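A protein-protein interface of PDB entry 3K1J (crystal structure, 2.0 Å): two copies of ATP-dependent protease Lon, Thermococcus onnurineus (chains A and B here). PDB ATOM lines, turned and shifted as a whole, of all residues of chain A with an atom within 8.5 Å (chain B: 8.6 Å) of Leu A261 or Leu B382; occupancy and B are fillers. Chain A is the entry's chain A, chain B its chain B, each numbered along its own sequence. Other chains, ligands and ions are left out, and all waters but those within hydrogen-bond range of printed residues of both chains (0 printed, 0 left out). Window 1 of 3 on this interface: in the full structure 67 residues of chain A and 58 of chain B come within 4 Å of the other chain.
No position is printed for both chains. Of the 9 pairs that touch across the chains among the printed residues, none has its exchanged pair printed and touching as well.
Of the 17 printed residues of chain B, 5 touch a printed residue of chain A. Along chain A the printed residues that touch a printed residue of chain B span positions 66 to 283.
N of Ile A66 is in hydrogen-bond range of O of Val A282, at 2.8 Å. The backbone carbonyl oxygen (O) of Ile A66 is in hydrogen-bond range of the backbone NH (N) of Met A284 (2.7 Å). The backbone carbonyl oxygen (O) of Lys B376 lies close to the side-chain amide oxygen (OE1) of Gln B381 (3.1 Å).
Of the printed residues of chain B, Ile A66 touches Leu B378. No residue of chain B comes within 4 Å of Asn A260. Leu A261 touches just one residue of chain B: Leu B382. Printed residues of chain B within 4 Å of Val A282: Gln B381 (3.7 Å). Printed residues of chain B within 4 Å of Tyr A283: Leu B378, Gln B381, Leu B382 and Trp B385. Printed residues of chain A within 4 Å of Leu B378: Ile A66 (3.4 Å), Val A264 (3.2 Å) and Tyr A283 (3.8 Å). Printed residues of chain A within 4 Å of Gln B381: Val A282 and Tyr A283. The nearest residue of chain A that does not touch Leu B382 is Ile A66 (6.0 Å). The nearest printed residue of chain A that does not touch Leu B378 is Val A282 (4.9 Å).
Ile A66 touches Leu B378 (CG1 to CD2, 3.4 Å). Leu A261 touches Leu B382. Leu B378 touches Val A264. CG1 of Val A264 touches OE2 of Glu B379, 3.7 Å away. Val A282 touches Gln B381. Tyr A283 touches Leu B378 (CB to CD1, 3.8 Å). CD1 of Leu B382 touches CZ of Tyr A283, at 3.9 Å. Tyr A283 touches Trp B385.
The backbone NH of Tyr A283 sits close to the side-chain amide nitrogen of Gln B381 (2.9 Å).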
ATOM      1  N   LEU A  65      13.988  -9.391 -27.848  1.00  0.00           N
ATOM      2  CA  LEU A  65      13.753  -7.962 -27.994  1.00  0.00           C
ATOM      3  C   LEU A  65      12.365  -7.619 -27.485  1.00  0.00           C
ATOM      4  O   LEU A  65      11.365  -8.057 -28.045  1.00  0.00           O
ATOM      5  CB  LEU A  65      13.883  -7.553 -29.471  1.00  0.00           C
ATOM      6  CG  LEU A  65      15.212  -7.865 -30.162  1.00  0.00           C
ATOM      7  CD1 LEU A  65      15.162  -7.377 -31.610  1.00  0.00           C
ATOM      8  CD2 LEU A  65      16.360  -7.185 -29.400  1.00  0.00           C
ATOM      9  N   ILE A  66      12.303  -6.826 -26.422  1.00  0.00           N
ATOM     10  CA  ILE A  66      11.025  -6.442 -25.846  1.00  0.00           C
ATOM     11  C   ILE A  66      10.735  -4.965 -26.087  1.00  0.00           C
ATOM     12  O   ILE A  66      11.532  -4.102 -25.720  1.00  0.00           O
ATOM     13  CB  ILE A  66      11.017  -6.722 -24.318  1.00  0.00           C
ATOM     14  CG1 ILE A  66      11.194  -8.222 -24.068  1.00  0.00           C
ATOM     15  CG2 ILE A  66       9.719  -6.223 -23.682  1.00  0.00           C
ATOM     16  CD1 ILE A  66      10.095  -9.086 -24.702  1.00  0.00           C
ATOM     17  N   GLY A  67       9.590  -4.674 -26.701  1.00  0.00           N
ATOM     18  CA  GLY A  67       9.236  -3.287 -26.948  1.00  0.00           C
ATOM     19  C   GLY A  67       7.883  -3.099 -27.611  1.00  0.00           C
ATOM     20  O   GLY A  67       7.233  -4.073 -27.996  1.00  0.00           O
ATOM     21  N   GLU A  68       7.463  -1.841 -27.741  1.00  0.00           N
ATOM     22  CA  GLU A  68       6.185  -1.499 -28.380  1.00  0.00           C
ATOM     23  C   GLU A  68       6.238  -1.888 -29.845  1.00  0.00           C
ATOM     24  O   GLU A  68       7.312  -1.987 -30.419  1.00  0.00           O
ATOM     25  CB  GLU A  68       5.931   0.010 -28.311  1.00  0.00           C
ATOM     26  CG  GLU A  68       5.734   0.582 -26.924  1.00  0.00           C
ATOM     27  CD  GLU A  68       5.418   2.071 -26.961  1.00  0.00           C
ATOM     28  OE1 GLU A  68       5.147   2.606 -28.063  1.00  0.00           O
ATOM     29  OE2 GLU A  68       5.435   2.710 -25.889  1.00  0.00           O
ATOM     30  N   PRO A  69       5.077  -2.113 -30.477  1.00  0.00           N
ATOM     31  CA  PRO A  69       5.142  -2.481 -31.895  1.00  0.00           C
ATOM     32  C   PRO A  69       5.649  -1.310 -32.745  1.00  0.00           C
ATOM     33  O   PRO A  69       5.455  -0.146 -32.385  1.00  0.00           O
ATOM     34  CB  PRO A  69       3.694  -2.855 -32.226  1.00  0.00           C
ATOM     35  CG  PRO A  69       2.896  -2.021 -31.272  1.00  0.00           C
ATOM     36  CD  PRO A  69       3.686  -2.122 -29.984  1.00  0.00           C
ATOM     37  N   LYS A  73      11.985  -3.991 -33.975  1.00  0.00           N
ATOM     38  CA  LYS A  73      12.420  -5.316 -33.541  1.00  0.00           C
ATOM     39  C   LYS A  73      12.711  -6.230 -34.731  1.00  0.00           C
ATOM     40  O   LYS A  73      13.774  -6.838 -34.809  1.00  0.00           O
ATOM     41  CB  LYS A  73      11.369  -5.939 -32.601  1.00  0.00           C
ATOM     42  CG  LYS A  73      11.137  -5.087 -31.351  1.00  0.00           C
ATOM     43  CD  LYS A  73      10.190  -5.733 -30.329  1.00  0.00           C
ATOM     44  CE  LYS A  73       8.789  -5.969 -30.898  1.00  0.00           C
ATOM     45  NZ  LYS A  73       8.104  -4.710 -31.316  1.00  0.00           N
ATOM     46  N   ALA A 211       5.517 -15.330 -26.848  1.00  0.00           N
ATOM     47  CA  ALA A 211       4.739 -15.881 -25.742  1.00  0.00           C
ATOM     48  C   ALA A 211       3.381 -16.422 -26.166  1.00  0.00           C
ATOM     49  O   ALA A 211       2.737 -17.130 -25.400  1.00  0.00           O
ATOM     50  CB  ALA A 211       4.560 -14.819 -24.643  1.00  0.00           C
ATOM     51  N   ALA A 258      10.747 -11.747 -29.976  1.00  0.00           N
ATOM     52  CA  ALA A 258      10.297 -10.402 -29.662  1.00  0.00           C
ATOM     53  C   ALA A 258       8.907 -10.419 -29.028  1.00  0.00           C
ATOM     54  O   ALA A 258       8.216 -11.429 -29.071  1.00  0.00           O
ATOM     55  CB  ALA A 258      10.288  -9.543 -30.934  1.00  0.00           C
ATOM     56  N   GLY A 259       8.517  -9.294 -28.436  1.00  0.00           N
ATOM     57  CA  GLY A 259       7.208  -9.175 -27.811  1.00  0.00           C
ATOM     58  C   GLY A 259       7.116  -7.863 -27.050  1.00  0.00           C
ATOM     59  O   GLY A 259       8.045  -7.054 -27.113  1.00  0.00           O
ATOM     60  N   ASN A 260       6.007  -7.626 -26.353  1.00  0.00           N
ATOM     61  CA  ASN A 260       5.870  -6.400 -25.569  1.00  0.00           C
ATOM     62  C   ASN A 260       6.015  -6.811 -24.110  1.00  0.00           C
ATOM     63  O   ASN A 260       6.352  -7.957 -23.825  1.00  0.00           O
ATOM     64  CB  ASN A 260       4.513  -5.718 -25.785  1.00  0.00           C
ATOM     65  CG  ASN A 260       4.582  -4.178 -25.604  1.00  0.00           C
ATOM     66  OD1 ASN A 260       5.473  -3.635 -24.908  1.00  0.00           O
ATOM     67  ND2 ASN A 260       3.632  -3.471 -26.225  1.00  0.00           N
ATOM     68  N   LEU A 261       5.759  -5.896 -23.188  1.00  0.00           N
ATOM     69  CA  LEU A 261       5.910  -6.198 -21.772  1.00  0.00           C
ATOM     70  C   LEU A 261       5.171  -7.421 -21.209  1.00  0.00           C
ATOM     71  O   LEU A 261       5.646  -8.026 -20.252  1.00  0.00           O
ATOM     72  CB  LEU A 261       5.567  -4.957 -20.958  1.00  0.00           C
ATOM     73  CG  LEU A 261       6.564  -3.852 -21.299  1.00  0.00           C
ATOM     74  CD1 LEU A 261       6.169  -2.543 -20.653  1.00  0.00           C
ATOM     75  CD2 LEU A 261       7.943  -4.295 -20.855  1.00  0.00           C
ATOM     76  N   ASP A 262       4.034  -7.797 -21.790  1.00  0.00           N
ATOM     77  CA  ASP A 262       3.284  -8.959 -21.296  1.00  0.00           C
ATOM     78  C   ASP A 262       4.020 -10.268 -21.602  1.00  0.00           C
ATOM     79  O   ASP A 262       3.919 -11.248 -20.868  1.00  0.00           O
ATOM     80  CB  ASP A 262       1.874  -8.988 -21.918  1.00  0.00           C
ATOM     81  CG  ASP A 262       1.793  -9.818 -23.220  1.00  0.00           C
ATOM     82  OD1 ASP A 262       2.781  -9.910 -23.983  1.00  0.00           O
ATOM     83  OD2 ASP A 262       0.703 -10.369 -23.497  1.00  0.00           O
ATOM     84  N   THR A 263       4.780 -10.258 -22.685  1.00  0.00           N
ATOM     85  CA  THR A 263       5.513 -11.427 -23.136  1.00  0.00           C
ATOM     86  C   THR A 263       6.421 -12.013 -22.066  1.00  0.00           C
ATOM     87  O   THR A 263       6.455 -13.224 -21.837  1.00  0.00           O
ATOM     88  CB  THR A 263       6.362 -11.068 -24.369  1.00  0.00           C
ATOM     89  OG1 THR A 263       5.506 -10.571 -25.407  1.00  0.00           O
ATOM     90  CG2 THR A 263       7.112 -12.287 -24.871  1.00  0.00           C
ATOM     91  N   VAL A 264       7.161 -11.135 -21.412  1.00  0.00           N
ATOM     92  CA  VAL A 264       8.093 -11.551 -20.384  1.00  0.00           C
ATOM     93  C   VAL A 264       7.550 -12.639 -19.448  1.00  0.00           C
ATOM     94  O   VAL A 264       8.112 -13.733 -19.362  1.00  0.00           O
ATOM     95  CB  VAL A 264       8.520 -10.344 -19.539  1.00  0.00           C
ATOM     96  CG1 VAL A 264       9.860 -10.631 -18.865  1.00  0.00           C
ATOM     97  CG2 VAL A 264       8.568  -9.090 -20.424  1.00  0.00           C
ATOM     98  N   ASP A 265       6.454 -12.335 -18.760  1.00  0.00           N
ATOM     99  CA  ASP A 265       5.877 -13.277 -17.814  1.00  0.00           C
ATOM    100  C   ASP A 265       5.029 -14.397 -18.407  1.00  0.00           C
ATOM    101  O   ASP A 265       4.754 -15.377 -17.720  1.00  0.00           O
ATOM    102  CB  ASP A 265       5.065 -12.523 -16.755  1.00  0.00           C
ATOM    103  CG  ASP A 265       5.919 -11.557 -15.942  1.00  0.00           C
ATOM    104  OD1 ASP A 265       7.034 -11.950 -15.529  1.00  0.00           O
ATOM    105  OD2 ASP A 265       5.475 -10.409 -15.706  1.00  0.00           O
ATOM    106  N   LYS A 266       4.623 -14.277 -19.668  1.00  0.00           N
ATOM    107  CA  LYS A 266       3.805 -15.323 -20.279  1.00  0.00           C
ATOM    108  C   LYS A 266       4.570 -16.408 -21.023  1.00  0.00           C
ATOM    109  O   LYS A 266       4.053 -17.504 -21.213  1.00  0.00           O
ATOM    110  CB  LYS A 266       2.786 -14.728 -21.246  1.00  0.00           C
ATOM    111  CG  LYS A 266       1.714 -13.886 -20.606  1.00  0.00           C
ATOM    112  CD  LYS A 266       0.693 -13.482 -21.660  1.00  0.00           C
ATOM    113  CE  LYS A 266      -0.406 -12.606 -21.084  1.00  0.00           C
ATOM    114  NZ  LYS A 266      -1.417 -12.268 -22.130  1.00  0.00           N
ATOM    115  N   MET A 267       5.794 -16.124 -21.453  1.00  0.00           N
ATOM    116  CA  MET A 267       6.535 -17.132 -22.195  1.00  0.00           C
ATOM    117  C   MET A 267       7.079 -18.263 -21.324  1.00  0.00           C
ATOM    118  O   MET A 267       7.243 -18.125 -20.110  1.00  0.00           O
ATOM    119  CB  MET A 267       7.664 -16.480 -23.006  1.00  0.00           C
ATOM    120  CG  MET A 267       8.808 -15.903 -22.205  1.00  0.00           C
ATOM    121  SD  MET A 267      10.016 -14.999 -23.272  1.00  0.00           S
ATOM    122  CE  MET A 267      10.668 -16.293 -24.186  1.00  0.00           C
ATOM    123  N   VAL A 282      16.798  -7.347 -24.491  1.00  0.00           N
ATOM    124  CA  VAL A 282      16.884  -5.925 -24.746  1.00  0.00           C
ATOM    125  C   VAL A 282      15.519  -5.252 -24.657  1.00  0.00           C
ATOM    126  O   VAL A 282      14.538  -5.760 -25.180  1.00  0.00           O
ATOM    127  CB  VAL A 282      17.453  -5.666 -26.153  1.00  0.00           C
ATOM    128  CG1 VAL A 282      17.535  -4.168 -26.408  1.00  0.00           C
ATOM    129  CG2 VAL A 282      18.831  -6.315 -26.290  1.00  0.00           C
ATOM    130  N   TYR A 283      15.448  -4.119 -23.972  1.00  0.00           N
ATOM    131  CA  TYR A 283      14.195  -3.389 -23.909  1.00  0.00           C
ATOM    132  C   TYR A 283      14.322  -2.223 -24.897  1.00  0.00           C
ATOM    133  O   TYR A 283      15.204  -1.378 -24.753  1.00  0.00           O
ATOM    134  CB  TYR A 283      13.931  -2.862 -22.496  1.00  0.00           C
ATOM    135  CG  TYR A 283      12.675  -2.026 -22.399  1.00  0.00           C
ATOM    136  CD1 TYR A 283      11.481  -2.467 -22.957  1.00  0.00           C
ATOM    137  CD2 TYR A 283      12.681  -0.801 -21.735  1.00  0.00           C
ATOM    138  CE1 TYR A 283      10.312  -1.707 -22.857  1.00  0.00           C
ATOM    139  CE2 TYR A 283      11.527  -0.031 -21.623  1.00  0.00           C
ATOM    140  CZ  TYR A 283      10.343  -0.492 -22.188  1.00  0.00           C
ATOM    141  OH  TYR A 283       9.205   0.265 -22.080  1.00  0.00           O
ATOM    142  N   MET A 284      13.452  -2.190 -25.900  1.00  0.00           N
ATOM    143  CA  MET A 284      13.484  -1.139 -26.916  1.00  0.00           C
ATOM    144  C   MET A 284      13.115   0.228 -26.359  1.00  0.00           C
ATOM    145  O   MET A 284      12.099   0.375 -25.685  1.00  0.00           O
ATOM    146  CB  MET A 284      12.512  -1.471 -28.052  1.00  0.00           C
ATOM    147  CG  MET A 284      12.714  -2.827 -28.691  1.00  0.00           C
ATOM    148  SD  MET A 284      14.312  -2.979 -29.477  1.00  0.00           S
ATOM    149  CE  MET A 284      14.030  -1.913 -30.934  1.00  0.00           C
ATOM    150  N   LYS B 376      21.749  -6.764 -18.364  1.00  0.00           N
ATOM    151  CA  LYS B 376      20.846  -6.762 -17.237  1.00  0.00           C
ATOM    152  C   LYS B 376      19.494  -7.367 -17.555  1.00  0.00           C
ATOM    153  O   LYS B 376      19.073  -7.435 -18.711  1.00  0.00           O
ATOM    154  CB  LYS B 376      20.654  -5.354 -16.639  1.00  0.00           C
ATOM    155  CG  LYS B 376      20.880  -4.163 -17.536  1.00  0.00           C
ATOM    156  CD  LYS B 376      20.752  -2.889 -16.700  1.00  0.00           C
ATOM    157  CE  LYS B 376      21.192  -1.660 -17.469  1.00  0.00           C
ATOM    158  NZ  LYS B 376      20.992  -0.408 -16.685  1.00  0.00           N
ATOM    159  N   PRO B 377      18.803  -7.838 -16.514  1.00  0.00           N
ATOM    160  CA  PRO B 377      17.483  -8.444 -16.650  1.00  0.00           C
ATOM    161  C   PRO B 377      16.531  -7.416 -17.248  1.00  0.00           C
ATOM    162  O   PRO B 377      16.575  -6.237 -16.905  1.00  0.00           O
ATOM    163  CB  PRO B 377      17.090  -8.770 -15.208  1.00  0.00           C
ATOM    164  CG  PRO B 377      18.405  -8.884 -14.500  1.00  0.00           C
ATOM    165  CD  PRO B 377      19.220  -7.792 -15.103  1.00  0.00           C
ATOM    166  N   LEU B 378      15.675  -7.867 -18.144  1.00  0.00           N
ATOM    167  CA  LEU B 378      14.699  -6.986 -18.736  1.00  0.00           C
ATOM    168  C   LEU B 378      13.967  -6.197 -17.632  1.00  0.00           C
ATOM    169  O   LEU B 378      13.562  -5.044 -17.835  1.00  0.00           O
ATOM    170  CB  LEU B 378      13.720  -7.828 -19.537  1.00  0.00           C
ATOM    171  CG  LEU B 378      12.385  -7.209 -19.913  1.00  0.00           C
ATOM    172  CD1 LEU B 378      12.581  -5.961 -20.741  1.00  0.00           C
ATOM    173  CD2 LEU B 378      11.595  -8.248 -20.680  1.00  0.00           C
ATOM    174  N   GLU B 379      13.815  -6.818 -16.461  1.00  0.00           N
ATOM    175  CA  GLU B 379      13.135  -6.171 -15.335  1.00  0.00           C
ATOM    176  C   GLU B 379      13.884  -4.941 -14.841  1.00  0.00           C
ATOM    177  O   GLU B 379      13.267  -3.964 -14.405  1.00  0.00           O
ATOM    178  CB  GLU B 379      12.953  -7.144 -14.161  1.00  0.00           C
ATOM    179  CG  GLU B 379      11.949  -8.277 -14.385  1.00  0.00           C
ATOM    180  CD  GLU B 379      12.486  -9.393 -15.271  1.00  0.00           C
ATOM    181  OE1 GLU B 379      13.713  -9.414 -15.533  1.00  0.00           O
ATOM    182  OE2 GLU B 379      11.674 -10.258 -15.691  1.00  0.00           O
ATOM    183  N   LYS B 380      15.210  -4.988 -14.895  1.00  0.00           N
ATOM    184  CA  LYS B 380      15.988  -3.847 -14.456  1.00  0.00           C
ATOM    185  C   LYS B 380      16.019  -2.747 -15.519  1.00  0.00           C
ATOM    186  O   LYS B 380      15.926  -1.554 -15.184  1.00  0.00           O
ATOM    187  CB  LYS B 380      17.413  -4.266 -14.092  1.00  0.00           C
ATOM    188  CG  LYS B 380      18.229  -3.104 -13.543  1.00  0.00           C
ATOM    189  CD  LYS B 380      19.504  -3.560 -12.867  1.00  0.00           C
ATOM    190  CE  LYS B 380      20.385  -2.363 -12.511  1.00  0.00           C
ATOM    191  NZ  LYS B 380      19.696  -1.395 -11.620  1.00  0.00           N
ATOM    192  N   GLN B 381      16.151  -3.136 -16.791  1.00  0.00           N
ATOM    193  CA  GLN B 381      16.170  -2.160 -17.879  1.00  0.00           C
ATOM    194  C   GLN B 381      14.851  -1.408 -17.810  1.00  0.00           C
ATOM    195  O   GLN B 381      14.796  -0.203 -18.047  1.00  0.00           O
ATOM    196  CB  GLN B 381      16.295  -2.842 -19.252  1.00  0.00           C
ATOM    197  CG  GLN B 381      17.530  -3.706 -19.418  1.00  0.00           C
ATOM    198  CD  GLN B 381      17.598  -4.381 -20.772  1.00  0.00           C
ATOM    199  OE1 GLN B 381      17.894  -5.575 -20.862  1.00  0.00           O
ATOM    200  NE2 GLN B 381      17.341  -3.624 -21.838  1.00  0.00           N
ATOM    201  N   LEU B 382      13.793  -2.134 -17.461  1.00  0.00           N
ATOM    202  CA  LEU B 382      12.464  -1.558 -17.352  1.00  0.00           C
ATOM    203  C   LEU B 382      12.415  -0.550 -16.210  1.00  0.00           C
ATOM    204  O   LEU B 382      11.885   0.546 -16.365  1.00  0.00           O
ATOM    205  CB  LEU B 382      11.433  -2.650 -17.091  1.00  0.00           C
ATOM    206  CG  LEU B 382       9.997  -2.296 -17.478  1.00  0.00           C
ATOM    207  CD1 LEU B 382       9.833  -2.550 -18.973  1.00  0.00           C
ATOM    208  CD2 LEU B 382       9.004  -3.144 -16.691  1.00  0.00           C
ATOM    209  N   ALA B 383      12.958  -0.935 -15.060  1.00  0.00           N
ATOM    210  CA  ALA B 383      12.972  -0.062 -13.895  1.00  0.00           C
ATOM    211  C   ALA B 383      13.848   1.161 -14.170  1.00  0.00           C
ATOM    212  O   ALA B 383      13.485   2.287 -13.828  1.00  0.00           O
ATOM    213  CB  ALA B 383      13.495  -0.829 -12.675  1.00  0.00           C
ATOM    214  N   ASP B 384      14.994   0.934 -14.801  1.00  0.00           N
ATOM    215  CA  ASP B 384      15.915   2.016 -15.112  1.00  0.00           C
ATOM    216  C   ASP B 384      15.308   2.986 -16.112  1.00  0.00           C
ATOM    217  O   ASP B 384      15.500   4.196 -16.013  1.00  0.00           O
ATOM    218  CB  ASP B 384      17.223   1.463 -15.676  1.00  0.00           C
ATOM    219  CG  ASP B 384      18.122   0.871 -14.604  1.00  0.00           C
ATOM    220  OD1 ASP B 384      17.785   0.973 -13.403  1.00  0.00           O
ATOM    221  OD2 ASP B 384      19.172   0.300 -14.970  1.00  0.00           O
ATOM    222  N   TRP B 385      14.591   2.443 -17.087  1.00  0.00           N
ATOM    223  CA  TRP B 385      13.947   3.265 -18.097  1.00  0.00           C
ATOM    224  C   TRP B 385      12.955   4.173 -17.383  1.00  0.00           C
ATOM    225  O   TRP B 385      12.934   5.379 -17.598  1.00  0.00           O
ATOM    226  CB  TRP B 385      13.218   2.372 -19.098  1.00  0.00           C
ATOM    227  CG  TRP B 385      12.355   3.118 -20.061  1.00  0.00           C
ATOM    228  CD1 TRP B 385      12.748   3.731 -21.225  1.00  0.00           C
ATOM    229  CD2 TRP B 385      10.949   3.355 -19.935  1.00  0.00           C
ATOM    230  NE1 TRP B 385      11.669   4.329 -21.828  1.00  0.00           N
ATOM    231  CE2 TRP B 385      10.552   4.113 -21.061  1.00  0.00           C
ATOM    232  CE3 TRP B 385       9.983   2.996 -18.984  1.00  0.00           C
ATOM    233  CZ2 TRP B 385       9.224   4.530 -21.254  1.00  0.00           C
ATOM    234  CZ3 TRP B 385       8.665   3.410 -19.176  1.00  0.00           C
ATOM    235  CH2 TRP B 385       8.298   4.166 -20.306  1.00  0.00           C
ATOM    236  N   TYR B 386      12.139   3.570 -16.524  1.00  0.00           N
ATOM    237  CA  TYR B 386      11.132   4.284 -15.744  1.00  0.00           C
ATOM    238  C   TYR B 386      11.745   5.376 -14.873  1.00  0.00           C
ATOM    239  O   TYR B 386      11.284   6.515 -14.881  1.00  0.00           O
ATOM    240  CB  TYR B 386      10.353   3.272 -14.888  1.00  0.00           C
ATOM    241  CG  TYR B 386       9.372   3.859 -13.901  1.00  0.00           C
ATOM    242  CD1 TYR B 386       9.740   4.077 -12.570  1.00  0.00           C
ATOM    243  CD2 TYR B 386       8.070   4.183 -14.286  1.00  0.00           C
ATOM    244  CE1 TYR B 386       8.839   4.595 -11.649  1.00  0.00           C
ATOM    245  CE2 TYR B 386       7.160   4.706 -13.372  1.00  0.00           C
ATOM    246  CZ  TYR B 386       7.555   4.907 -12.059  1.00  0.00           C
ATOM    247  OH  TYR B 386       6.675   5.435 -11.150  1.00  0.00           O
ATOM    248  N   ILE B 387      12.793   5.035 -14.133  1.00  0.00           N
ATOM    249  CA  ILE B 387      13.457   6.002 -13.267  1.00  0.00           C
ATOM    250  C   ILE B 387      14.027   7.158 -14.082  1.00  0.00           C
ATOM    251  O   ILE B 387      13.997   8.320 -13.659  1.00  0.00           O
ATOM    252  CB  ILE B 387      14.586   5.312 -12.468  1.00  0.00           C
ATOM    253  CG1 ILE B 387      13.963   4.435 -11.370  1.00  0.00           C
ATOM    254  CG2 ILE B 387      15.552   6.353 -11.888  1.00  0.00           C
ATOM    255  CD1 ILE B 387      14.932   3.461 -10.736  1.00  0.00           C
ATOM    256  N   GLU B 388      14.543   6.838 -15.259  1.00  0.00           N
ATOM    257  CA  GLU B 388      15.125   7.852 -16.127  1.00  0.00           C
ATOM    258  C   GLU B 388      14.055   8.811 -16.643  1.00  0.00           C
ATOM    259  O   GLU B 388      14.267  10.013 -16.701  1.00  0.00           O
ATOM    260  CB  GLU B 388      15.830   7.181 -17.305  1.00  0.00           C
ATOM    261  CG  GLU B 388      16.439   8.145 -18.301  1.00  0.00           C
ATOM    262  CD  GLU B 388      16.847   7.458 -19.592  1.00  0.00           C
ATOM    263  OE1 GLU B 388      17.539   6.424 -19.521  1.00  0.00           O
ATOM    264  OE2 GLU B 388      16.479   7.955 -20.676  1.00  0.00           O
ATOM    265  N   ARG B 389      12.904   8.273 -17.028  1.00  0.00           N
ATOM    266  CA  ARG B 389      11.819   9.108 -17.526  1.00  0.00           C
ATOM    267  C   ARG B 389      11.313  10.009 -16.414  1.00  0.00           C
ATOM    268  O   ARG B 389      11.048  11.188 -16.628  1.00  0.00           O
ATOM    269  CB  ARG B 389      10.670   8.236 -18.023  1.00  0.00           C
ATOM    270  CG  ARG B 389      11.105   7.207 -19.030  1.00  0.00           C
ATOM    271  CD  ARG B 389      11.499   7.843 -20.342  1.00  0.00           C
ATOM    272  NE  ARG B 389      10.311   8.273 -21.073  1.00  0.00           N
ATOM    273  CZ  ARG B 389      10.194   8.251 -22.398  1.00  0.00           C
ATOM    274  NH1 ARG B 389      11.201   7.818 -23.151  1.00  0.00           N
ATOM    275  NH2 ARG B 389       9.062   8.649 -22.965  1.00  0.00           N
ATOM    276  N   ILE B 412      12.531   0.524  -6.946  1.00  0.00           N
ATOM    277  CA  ILE B 412      11.591   0.048  -7.947  1.00  0.00           C
ATOM    278  C   ILE B 412      12.024  -1.345  -8.385  1.00  0.00           C
ATOM    279  O   ILE B 412      13.117  -1.524  -8.927  1.00  0.00           O
ATOM    280  CB  ILE B 412      11.587   0.958  -9.184  1.00  0.00           C
ATOM    281  CG1 ILE B 412      11.419   2.420  -8.764  1.00  0.00           C
ATOM    282  CG2 ILE B 412      10.468   0.530 -10.134  1.00  0.00           C
ATOM    283  CD1 ILE B 412      10.135   2.720  -8.003  1.00  0.00           C
ATOM    284  N   GLY B 413      11.174  -2.336  -8.147  1.00  0.00           N
ATOM    285  CA  GLY B 413      11.536  -3.685  -8.534  1.00  0.00           C
ATOM    286  C   GLY B 413      12.473  -4.308  -7.517  1.00  0.00           C
ATOM    287  O   GLY B 413      12.147  -4.383  -6.333  1.00  0.00           O
ATOM    288  N   SER B 416      16.731  -1.107  -8.346  1.00  0.00           N
ATOM    289  CA  SER B 416      16.746   0.218  -8.952  1.00  0.00           C
ATOM    290  C   SER B 416      16.080   1.260  -8.063  1.00  0.00           C
ATOM    291  O   SER B 416      14.887   1.179  -7.772  1.00  0.00           O
ATOM    292  CB  SER B 416      16.067   0.178 -10.313  1.00  0.00           C
ATOM    293  OG  SER B 416      16.885  -0.503 -11.242  1.00  0.00           O
